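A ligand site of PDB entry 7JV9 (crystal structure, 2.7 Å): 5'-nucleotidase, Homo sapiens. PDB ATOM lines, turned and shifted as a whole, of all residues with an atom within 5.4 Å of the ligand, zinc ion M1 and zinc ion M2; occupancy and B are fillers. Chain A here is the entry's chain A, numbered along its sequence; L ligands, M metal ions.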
ATOM      1  N   ASP A  12      18.404 -10.693  30.830  1.00  0.00           N
ATOM      2  CA  ASP A  12      18.466 -11.401  29.538  1.00  0.00           C
ATOM      3  C   ASP A  12      19.772 -11.156  28.777  1.00  0.00           C
ATOM      4  O   ASP A  12      19.775 -10.961  27.559  1.00  0.00           O
ATOM      5  CB  ASP A  12      17.247 -11.022  28.693  1.00  0.00           C
ATOM      6  CG  ASP A  12      15.981 -11.630  29.229  1.00  0.00           C
ATOM      7  OD1 ASP A  12      15.755 -12.842  29.022  1.00  0.00           O
ATOM      8  OD2 ASP A  12      15.203 -10.903  29.858  1.00  0.00           O
ATOM      9  N   HIS A  14      22.040 -13.355  28.257  1.00  0.00           N
ATOM     10  CA  HIS A  14      22.164 -14.532  27.377  1.00  0.00           C
ATOM     11  C   HIS A  14      23.595 -14.847  26.891  1.00  0.00           C
ATOM     12  O   HIS A  14      23.858 -14.997  25.703  1.00  0.00           O
ATOM     13  CB  HIS A  14      21.264 -14.387  26.155  1.00  0.00           C
ATOM     14  CG  HIS A  14      19.818 -14.607  26.443  1.00  0.00           C
ATOM     15  ND1 HIS A  14      19.345 -15.689  27.150  1.00  0.00           N
ATOM     16  CD2 HIS A  14      18.732 -13.892  26.064  1.00  0.00           C
ATOM     17  CE1 HIS A  14      18.021 -15.637  27.166  1.00  0.00           C
ATOM     18  NE2 HIS A  14      17.643 -14.480  26.645  1.00  0.00           N
ATOM     19  N   ASP A  61      18.247 -15.042  33.102  1.00  0.00           N
ATOM     20  CA  ASP A  61      18.620 -15.394  31.720  1.00  0.00           C
ATOM     21  C   ASP A  61      20.051 -14.926  31.357  1.00  0.00           C
ATOM     22  O   ASP A  61      20.314 -14.430  30.257  1.00  0.00           O
ATOM     23  CB  ASP A  61      17.551 -14.920  30.697  1.00  0.00           C
ATOM     24  CG  ASP A  61      16.307 -15.862  30.635  1.00  0.00           C
ATOM     25  OD1 ASP A  61      16.175 -16.742  31.515  1.00  0.00           O
ATOM     26  OD2 ASP A  61      15.454 -15.678  29.713  1.00  0.00           O
ATOM     27  N   GLN A  64      22.745 -19.433  28.758  1.00  0.00           N
ATOM     28  CA  GLN A  64      22.322 -19.778  27.392  1.00  0.00           C
ATOM     29  C   GLN A  64      22.359 -18.609  26.411  1.00  0.00           C
ATOM     30  O   GLN A  64      21.734 -17.563  26.638  1.00  0.00           O
ATOM     31  CB  GLN A  64      20.950 -20.456  27.394  1.00  0.00           C
ATOM     32  CG  GLN A  64      20.655 -21.306  26.162  1.00  0.00           C
ATOM     33  CD  GLN A  64      19.651 -20.653  25.196  1.00  0.00           C
ATOM     34  OE1 GLN A  64      19.648 -19.429  24.999  1.00  0.00           O
ATOM     35  NE2 GLN A  64      18.807 -21.492  24.575  1.00  0.00           N
ATOM     36  N   ASN A  93      14.455 -18.464  33.709  1.00  0.00           N
ATOM     37  CA  ASN A  93      14.027 -19.737  33.153  1.00  0.00           C
ATOM     38  C   ASN A  93      15.167 -20.491  32.444  1.00  0.00           C
ATOM     39  O   ASN A  93      15.187 -21.729  32.418  1.00  0.00           O
ATOM     40  CB  ASN A  93      12.810 -19.582  32.237  1.00  0.00           C
ATOM     41  CG  ASN A  93      13.117 -18.821  30.975  1.00  0.00           C
ATOM     42  OD1 ASN A  93      13.186 -17.589  30.964  1.00  0.00           O
ATOM     43  ND2 ASN A  93      13.273 -19.542  29.874  1.00  0.00           N
ATOM     44  N   HIS A  94      16.101 -19.743  31.881  1.00  0.00           N
ATOM     45  CA  HIS A  94      17.267 -20.354  31.220  1.00  0.00           C
ATOM     46  C   HIS A  94      18.346 -20.885  32.156  1.00  0.00           C
ATOM     47  O   HIS A  94      19.175 -21.708  31.756  1.00  0.00           O
ATOM     48  CB  HIS A  94      17.868 -19.411  30.183  1.00  0.00           C
ATOM     49  CG  HIS A  94      17.118 -19.420  28.884  1.00  0.00           C
ATOM     50  ND1 HIS A  94      17.261 -20.412  27.943  1.00  0.00           N
ATOM     51  CD2 HIS A  94      16.173 -18.574  28.401  1.00  0.00           C
ATOM     52  CE1 HIS A  94      16.477 -20.151  26.913  1.00  0.00           C
ATOM     53  NE2 HIS A  94      15.801 -19.048  27.167  1.00  0.00           N
ATOM     54  N   ASP A  97      18.395 -24.671  32.206  1.00  0.00           N
ATOM     55  CA  ASP A  97      18.637 -25.355  30.923  1.00  0.00           C
ATOM     56  C   ASP A  97      19.476 -26.622  31.081  1.00  0.00           C
ATOM     57  O   ASP A  97      19.104 -27.672  30.540  1.00  0.00           O
ATOM     58  CB  ASP A  97      19.305 -24.411  29.908  1.00  0.00           C
ATOM     59  CG  ASP A  97      18.330 -23.417  29.323  1.00  0.00           C
ATOM     60  OD1 ASP A  97      17.128 -23.459  29.679  1.00  0.00           O
ATOM     61  OD2 ASP A  97      18.748 -22.586  28.491  1.00  0.00           O
ATOM     62  N   PHE A 159       7.816 -25.543  31.151  1.00  0.00           N
ATOM     63  CA  PHE A 159       7.481 -25.768  29.720  1.00  0.00           C
ATOM     64  C   PHE A 159       8.574 -25.237  28.769  1.00  0.00           C
ATOM     65  O   PHE A 159       8.573 -25.573  27.588  1.00  0.00           O
ATOM     66  CB  PHE A 159       6.127 -25.117  29.333  1.00  0.00           C
ATOM     67  CG  PHE A 159       5.022 -25.385  30.304  1.00  0.00           C
ATOM     68  CD1 PHE A 159       4.366 -26.616  30.338  1.00  0.00           C
ATOM     69  CD2 PHE A 159       4.616 -24.405  31.200  1.00  0.00           C
ATOM     70  CE1 PHE A 159       3.341 -26.867  31.239  1.00  0.00           C
ATOM     71  CE2 PHE A 159       3.599 -24.639  32.114  1.00  0.00           C
ATOM     72  CZ  PHE A 159       2.963 -25.876  32.136  1.00  0.00           C
ATOM     73  N   LEU A 160       9.463 -24.408  29.307  1.00  0.00           N
ATOM     74  CA  LEU A 160      10.540 -23.733  28.538  1.00  0.00           C
ATOM     75  C   LEU A 160      11.949 -24.192  28.887  1.00  0.00           C
ATOM     76  O   LEU A 160      12.899 -23.679  28.312  1.00  0.00           O
ATOM     77  CB  LEU A 160      10.495 -22.236  28.757  1.00  0.00           C
ATOM     78  CG  LEU A 160       9.213 -21.512  28.365  1.00  0.00           C
ATOM     79  CD1 LEU A 160       9.345 -20.046  28.759  1.00  0.00           C
ATOM     80  CD2 LEU A 160       8.911 -21.655  26.887  1.00  0.00           C
ATOM     81  N   SER A 161      12.095 -25.119  29.815  1.00  0.00           N
ATOM     82  CA  SER A 161      13.417 -25.515  30.297  1.00  0.00           C
ATOM     83  C   SER A 161      13.353 -26.878  30.972  1.00  0.00           C
ATOM     84  O   SER A 161      12.453 -27.680  30.683  1.00  0.00           O
ATOM     85  CB  SER A 161      13.964 -24.449  31.238  1.00  0.00           C
ATOM     86  OG  SER A 161      15.365 -24.578  31.357  1.00  0.00           O
ATOM     87  N   ASN A 162      14.320 -27.152  31.848  1.00  0.00           N
ATOM     88  CA  ASN A 162      14.477 -28.464  32.489  1.00  0.00           C
ATOM     89  C   ASN A 162      14.729 -28.369  34.012  1.00  0.00           C
ATOM     90  O   ASN A 162      15.736 -28.849  34.518  1.00  0.00           O
ATOM     91  CB  ASN A 162      15.605 -29.223  31.761  1.00  0.00           C
ATOM     92  CG  ASN A 162      15.623 -30.714  32.042  1.00  0.00           C
ATOM     93  OD1 ASN A 162      14.665 -31.270  32.582  1.00  0.00           O
ATOM     94  ND2 ASN A 162      16.719 -31.361  31.685  1.00  0.00           N
ATOM     95  N   HIS A 196      11.906 -12.625  37.048  1.00  0.00           N
ATOM     96  CA  HIS A 196      11.963 -13.047  35.648  1.00  0.00           C
ATOM     97  C   HIS A 196      10.646 -13.636  35.120  1.00  0.00           C
ATOM     98  O   HIS A 196      10.573 -14.803  34.805  1.00  0.00           O
ATOM     99  CB  HIS A 196      13.083 -14.064  35.491  1.00  0.00           C
ATOM    100  CG  HIS A 196      13.482 -14.304  34.083  1.00  0.00           C
ATOM    101  ND1 HIS A 196      14.376 -13.492  33.417  1.00  0.00           N
ATOM    102  CD2 HIS A 196      13.076 -15.219  33.199  1.00  0.00           C
ATOM    103  CE1 HIS A 196      14.557 -13.937  32.198  1.00  0.00           C
ATOM    104  NE2 HIS A 196      13.658 -14.924  31.989  1.00  0.00           N
ATOM    105  N   HIS A 219      12.906 -11.219  31.141  1.00  0.00           N
ATOM    106  CA  HIS A 219      12.183 -12.320  30.410  1.00  0.00           C
ATOM    107  C   HIS A 219      11.541 -11.902  29.083  1.00  0.00           C
ATOM    108  O   HIS A 219      11.773 -12.555  28.059  1.00  0.00           O
ATOM    109  CB  HIS A 219      11.166 -13.037  31.314  1.00  0.00           C
ATOM    110  CG  HIS A 219      10.580 -14.289  30.734  1.00  0.00           C
ATOM    111  ND1 HIS A 219      11.326 -15.316  30.156  1.00  0.00           N
ATOM    112  CD2 HIS A 219       9.272 -14.628  30.522  1.00  0.00           C
ATOM    113  CE1 HIS A 219      10.499 -16.273  29.760  1.00  0.00           C
ATOM    114  NE2 HIS A 219       9.261 -15.879  29.953  1.00  0.00           N
ATOM    115  N   ASN A 221      12.197  -9.156  27.303  1.00  0.00           N
ATOM    116  CA  ASN A 221      13.138  -8.362  26.456  1.00  0.00           C
ATOM    117  C   ASN A 221      12.642  -6.922  26.191  1.00  0.00           C
ATOM    118  O   ASN A 221      12.839  -6.356  25.103  1.00  0.00           O
ATOM    119  CB  ASN A 221      13.484  -9.111  25.140  1.00  0.00           C
ATOM    120  CG  ASN A 221      14.478 -10.266  25.347  1.00  0.00           C
ATOM    121  OD1 ASN A 221      14.490 -10.915  26.379  1.00  0.00           O
ATOM    122  ND2 ASN A 221      15.284 -10.544  24.332  1.00  0.00           N
ATOM    123  N   ARG A 330       9.488 -13.722  14.835  1.00  0.00           N
ATOM    124  CA  ARG A 330       8.260 -13.922  15.614  1.00  0.00           C
ATOM    125  C   ARG A 330       7.022 -13.240  15.042  1.00  0.00           C
ATOM    126  O   ARG A 330       5.887 -13.593  15.392  1.00  0.00           O
ATOM    127  CB  ARG A 330       8.481 -13.437  17.030  1.00  0.00           C
ATOM    128  CG  ARG A 330       9.684 -14.089  17.684  1.00  0.00           C
ATOM    129  CD  ARG A 330       9.718 -13.828  19.179  1.00  0.00           C
ATOM    130  NE  ARG A 330      10.809 -14.568  19.820  1.00  0.00           N
ATOM    131  CZ  ARG A 330      10.924 -14.786  21.128  1.00  0.00           C
ATOM    132  NH1 ARG A 330      10.039 -14.305  22.002  1.00  0.00           N
ATOM    133  NH2 ARG A 330      11.957 -15.487  21.568  1.00  0.00           N
ATOM    134  N   ASN A 366       9.528 -23.121  15.103  1.00  0.00           N
ATOM    135  CA  ASN A 366       9.127 -22.061  16.050  1.00  0.00           C
ATOM    136  C   ASN A 366      10.113 -20.915  15.960  1.00  0.00           C
ATOM    137  O   ASN A 366      11.311 -21.098  16.191  1.00  0.00           O
ATOM    138  CB  ASN A 366       8.954 -22.560  17.508  1.00  0.00           C
ATOM    139  CG  ASN A 366      10.227 -23.123  18.116  1.00  0.00           C
ATOM    140  OD1 ASN A 366      10.844 -24.047  17.570  1.00  0.00           O
ATOM    141  ND2 ASN A 366      10.626 -22.586  19.268  1.00  0.00           N
ATOM    142  N   GLY A 367       9.611 -19.741  15.590  1.00  0.00           N
ATOM    143  CA  GLY A 367      10.430 -18.531  15.455  1.00  0.00           C
ATOM    144  C   GLY A 367      11.224 -18.159  16.691  1.00  0.00           C
ATOM    145  O   GLY A 367      12.336 -17.647  16.583  1.00  0.00           O
ATOM    146  N   GLY A 368      10.668 -18.428  17.860  1.00  0.00           N
ATOM    147  CA  GLY A 368      11.362 -18.224  19.131  1.00  0.00           C
ATOM    148  C   GLY A 368      12.616 -19.044  19.360  1.00  0.00           C
ATOM    149  O   GLY A 368      13.424 -18.728  20.236  1.00  0.00           O
ATOM    150  N   GLY A 369      12.762 -20.139  18.616  1.00  0.00           N
ATOM    151  CA  GLY A 369      13.984 -20.957  18.647  1.00  0.00           C
ATOM    152  C   GLY A 369      15.164 -20.365  17.898  1.00  0.00           C
ATOM    153  O   GLY A 369      16.288 -20.879  18.024  1.00  0.00           O
ATOM    154  N   ARG A 371      17.624 -17.494  17.540  1.00  0.00           N
ATOM    155  CA  ARG A 371      18.142 -16.686  18.648  1.00  0.00           C
ATOM    156  C   ARG A 371      19.196 -15.657  18.296  1.00  0.00           C
ATOM    157  O   ARG A 371      19.672 -14.915  19.150  1.00  0.00           O
ATOM    158  CB  ARG A 371      18.709 -17.656  19.674  1.00  0.00           C
ATOM    159  CG  ARG A 371      17.620 -18.427  20.380  1.00  0.00           C
ATOM    160  CD  ARG A 371      17.146 -17.655  21.597  1.00  0.00           C
ATOM    161  NE  ARG A 371      15.718 -17.669  21.836  1.00  0.00           N
ATOM    162  CZ  ARG A 371      15.155 -17.212  22.943  1.00  0.00           C
ATOM    163  NH1 ARG A 371      15.897 -16.664  23.909  1.00  0.00           N
ATOM    164  NH2 ARG A 371      13.845 -17.294  23.091  1.00  0.00           N
ATOM    165  N   PHE A 393      20.025 -24.088  21.817  1.00  0.00           N
ATOM    166  CA  PHE A 393      19.354 -25.132  22.599  1.00  0.00           C
ATOM    167  C   PHE A 393      19.995 -26.524  22.518  1.00  0.00           C
ATOM    168  O   PHE A 393      20.008 -27.265  23.505  1.00  0.00           O
ATOM    169  CB  PHE A 393      17.886 -25.233  22.187  1.00  0.00           C
ATOM    170  CG  PHE A 393      17.098 -23.990  22.508  1.00  0.00           C
ATOM    171  CD1 PHE A 393      16.570 -23.797  23.783  1.00  0.00           C
ATOM    172  CD2 PHE A 393      16.881 -23.007  21.543  1.00  0.00           C
ATOM    173  CE1 PHE A 393      15.838 -22.644  24.092  1.00  0.00           C
ATOM    174  CE2 PHE A 393      16.156 -21.863  21.843  1.00  0.00           C
ATOM    175  CZ  PHE A 393      15.624 -21.678  23.123  1.00  0.00           C
ATOM    176  N   THR A 422       5.775 -13.359  20.870  1.00  0.00           N
ATOM    177  CA  THR A 422       5.888 -14.700  21.421  1.00  0.00           C
ATOM    178  C   THR A 422       6.430 -15.654  20.349  1.00  0.00           C
ATOM    179  O   THR A 422       6.299 -15.411  19.133  1.00  0.00           O
ATOM    180  CB  THR A 422       4.563 -15.196  22.026  1.00  0.00           C
ATOM    181  OG1 THR A 422       3.464 -14.706  21.261  1.00  0.00           O
ATOM    182  CG2 THR A 422       4.430 -14.720  23.469  1.00  0.00           C
ATOM    183  N   GLY A 423       7.034 -16.747  20.839  1.00  0.00           N
ATOM    184  CA  GLY A 423       7.863 -17.636  20.030  1.00  0.00           C
ATOM    185  C   GLY A 423       7.179 -18.733  19.234  1.00  0.00           C
ATOM    186  O   GLY A 423       7.806 -19.343  18.383  1.00  0.00           O
ATOM    187  N   GLU A 424       5.898 -18.963  19.506  1.00  0.00           N
ATOM    188  CA  GLU A 424       5.090 -19.964  18.777  1.00  0.00           C
ATOM    189  C   GLU A 424       4.961 -19.709  17.260  1.00  0.00           C
ATOM    190  O   GLU A 424       4.746 -20.654  16.501  1.00  0.00           O
ATOM    191  CB  GLU A 424       3.692 -20.115  19.418  1.00  0.00           C
ATOM    192  CG  GLU A 424       2.745 -18.934  19.211  1.00  0.00           C
ATOM    193  CD  GLU A 424       2.456 -18.106  20.454  1.00  0.00           C
ATOM    194  OE1 GLU A 424       3.230 -18.173  21.435  1.00  0.00           O
ATOM    195  OE2 GLU A 424       1.435 -17.395  20.471  1.00  0.00           O
ATOM    196  N   PRO A 474      11.500 -29.095  15.046  1.00  0.00           N
ATOM    197  CA  PRO A 474      12.333 -29.332  16.224  1.00  0.00           C
ATOM    198  C   PRO A 474      11.658 -30.274  17.195  1.00  0.00           C
ATOM    199  O   PRO A 474      10.431 -30.336  17.238  1.00  0.00           O
ATOM    200  CB  PRO A 474      12.481 -27.939  16.854  1.00  0.00           C
ATOM    201  CG  PRO A 474      11.818 -26.987  15.947  1.00  0.00           C
ATOM    202  CD  PRO A 474      10.857 -27.772  15.117  1.00  0.00           C
ATOM    203  N   PHE A 476      11.493 -29.995  20.339  1.00  0.00           N
ATOM    204  CA  PHE A 476      10.741 -29.137  21.273  1.00  0.00           C
ATOM    205  C   PHE A 476       9.272 -29.061  20.899  1.00  0.00           C
ATOM    206  O   PHE A 476       8.394 -29.227  21.752  1.00  0.00           O
ATOM    207  CB  PHE A 476      11.350 -27.751  21.262  1.00  0.00           C
ATOM    208  CG  PHE A 476      10.579 -26.726  22.072  1.00  0.00           C
ATOM    209  CD1 PHE A 476      10.550 -26.797  23.471  1.00  0.00           C
ATOM    210  CD2 PHE A 476       9.914 -25.681  21.446  1.00  0.00           C
ATOM    211  CE1 PHE A 476       9.860 -25.840  24.220  1.00  0.00           C
ATOM    212  CE2 PHE A 476       9.228 -24.716  22.190  1.00  0.00           C
ATOM    213  CZ  PHE A 476       9.205 -24.800  23.572  1.00  0.00           C
ATOM    214  N   ASP A 482       5.913 -24.937  23.261  1.00  0.00           N
ATOM    215  CA  ASP A 482       5.274 -23.691  22.781  1.00  0.00           C
ATOM    216  C   ASP A 482       3.746 -23.782  22.716  1.00  0.00           C
ATOM    217  O   ASP A 482       3.106 -23.199  21.838  1.00  0.00           O
ATOM    218  CB  ASP A 482       5.876 -23.244  21.412  1.00  0.00           C
ATOM    219  CG  ASP A 482       6.724 -21.973  21.513  1.00  0.00           C
ATOM    220  OD1 ASP A 482       6.700 -21.266  22.539  1.00  0.00           O
ATOM    221  OD2 ASP A 482       7.414 -21.663  20.512  1.00  0.00           O
HETATM  222  C1  LIG L   1      15.597 -26.648  27.160  1.00  0.00           C
HETATM  223  C2  LIG L   1      16.194 -27.713  27.820  1.00  0.00           C
HETATM  224  C3  LIG L   1      15.522 -28.924  27.938  1.00  0.00           C
HETATM  225  C4  LIG L   1      14.258 -29.083  27.379  1.00  0.00           C
HETATM  226  C5  LIG L   1      13.668 -28.027  26.711  1.00  0.00           C
HETATM  227  C6  LIG L   1      14.329 -26.795  26.596  1.00  0.00           C
HETATM  228  C7  LIG L   1      13.634 -25.687  25.855  1.00  0.00           C
HETATM  229  C8  LIG L   1      13.354 -24.559  21.128  1.00  0.00           C
HETATM  230  C9  LIG L   1      12.447 -22.942  22.521  1.00  0.00           C
HETATM  231  C10 LIG L   1      12.700 -23.768  23.650  1.00  0.00           C
HETATM  232  C11 LIG L   1      12.233 -23.058  24.771  1.00  0.00           C
HETATM  233  C12 LIG L   1      10.453 -18.412  24.916  1.00  0.00           C
HETATM  234  O1  LIG L   1      13.142 -14.943  26.448  1.00  0.00           O
HETATM  235  O2  LIG L   1      13.424 -16.805  28.389  1.00  0.00           O
HETATM  236  C13 LIG L   1       9.325 -19.810  23.301  1.00  0.00           C
HETATM  237  C14 LIG L   1       9.853 -20.752  22.192  1.00  0.00           C
HETATM  238 CL1  LIG L   1      16.484 -25.150  27.051  1.00  0.00          CL
HETATM  239  N1  LIG L   1      13.629 -25.952  24.402  1.00  0.00           N
HETATM  240  C15 LIG L   1      13.320 -25.023  23.414  1.00  0.00           C
HETATM  241  N2  LIG L   1      13.607 -25.353  22.162  1.00  0.00           N
HETATM  242 CL2  LIG L   1      13.789 -25.144  19.544  1.00  0.00          CL
HETATM  243  N3  LIG L   1      12.784 -23.367  21.306  1.00  0.00           N
HETATM  244  N4  LIG L   1      11.741 -21.929  24.399  1.00  0.00           N
HETATM  245  N5  LIG L   1      11.859 -21.813  23.028  1.00  0.00           N
HETATM  246  C16 LIG L   1      11.393 -20.650  22.329  1.00  0.00           C
HETATM  247  O3  LIG L   1      11.685 -19.521  23.186  1.00  0.00           O
HETATM  248  C17 LIG L   1      10.472 -18.825  23.474  1.00  0.00           C
HETATM  249  O4  LIG L   1      11.374 -17.362  25.101  1.00  0.00           O
HETATM  250  C18 LIG L   1      11.369 -16.929  26.461  1.00  0.00           C
HETATM  251  P1  LIG L   1      13.066 -16.494  26.844  1.00  0.00           P
HETATM  252  O5  LIG L   1      14.038 -17.260  26.026  1.00  0.00           O
HETATM  253  O6  LIG L   1       8.137 -19.098  22.908  1.00  0.00           O
HETATM  254  O7  LIG L   1       9.455 -20.339  20.887  1.00  0.00           O
HETATM  255 ZN    ZN M   1      16.059 -14.629  27.978  1.00  0.00          ZN
HETATM  256 ZN    ZN M   2      13.377 -15.738  30.057  1.00  0.00          ZN
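Zinc ion M1 is bound by NE2 of His 14 (2.1 Å), OD1 of Asp 12 (2.1 Å) and OD2 of Asp 61 (2.1 Å).
OD1 of Asp 97 touches CL1 of the ligand, at 3.2 Å. Leu 160 touches the ligand. Ser 161 touches the ligand (CA to C1, 3.98 Å). Asn 162 touches the ligand (CB to C3, 3.8 Å). Gly 368 touches the ligand (CA to O7, 3.3 Å). CA of Gly 369 touches N3 of the ligand (3.8 Å). CE1 of Phe 393 touches C10 of the ligand (3.4 Å). Phe 476 touches the ligand. Of the 27 residues printed, 16 come within 4 Å of the ligand. The nearest printed residue that does not touch the ligand is Arg 330 (4.04 Å).
His 94 touches zinc ion M1 (CD2 to ZN, 3.97 Å).
The guanidinium group (NH1) of Arg 371 lies within salt-bridge range of an oxygen (O5) of the ligand (2.9 Å). The side-chain amide nitrogen (ND2) of Asn 366 is in hydrogen-bond range of an oxygen (O7) of the ligand (3.0 Å). An oxygen (O7) of the ligand sits at hydrogen-bond distance from the backbone carbonyl oxygen (O) of Gly 423, 3.2 Å away. An oxygen (O7) of the ligand lies within hydrogen-bond range of the side-chain carboxylate (OD2) of Asp 482 (2.5 Å). The backbone NH of Gly 423 lies close to an oxygen (O6) of the ligand, at 3.3 Å. A ring nitrogen (NE2) of His 94 lies within hydrogen-bond range of an oxygen (O5) of the ligand (2.8 Å).
OD2 of Asp 482 lies within hydrogen-bond range of N of Glu 424, at 3.3 Å. The side-chain amide nitrogen (ND2) of Asn 366 sits close to the backbone NH (N) of Gly 369 (3.3 Å). The backbone NH (N) of His 219 lies within hydrogen-bond range of the side-chain carboxylate (OD2) of Asp 12, 2.6 Å away. The backbone NH (N) of His 94 lies within hydrogen-bond range of the side-chain carboxylate (OD1) of Asp 61, 3.0 Å away. The guanidinium group (NE) of Arg 371 sits at hydrogen-bond distance from the backbone carbonyl oxygen (O) of Gly 368 (3.0 Å). The side-chain hydroxyl (OG) of Ser 161 sits at hydrogen-bond distance from the backbone carbonyl oxygen (O) of Asn 93, at 3.0 Å. ND1 of His 94 sits at hydrogen-bond distance from OD2 of Asp 97, 2.7 Å away. OD1 of Asp 97 lies within hydrogen-bond range of OG of Ser 161, 2.7 Å away.
Zinc ion M2 is bound by O2 of the ligand. The side-chain amide oxygen (OD1) of Asn 93 binds zinc ion M2, at 2.1 Å. Zinc ion M2 is bound by a ring nitrogen (ND1) of His 219, 2.1 Å away. Zinc ion M2 is bound by OD2 of Asp 61. NE2 of His 196 is bound to zinc ion M2, 2.1 Å away. Zinc ion M2 has five donor atoms within binding distance.
The nearest printed residue that does not touch zinc ion M2 is His 94 (4.3 Å).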
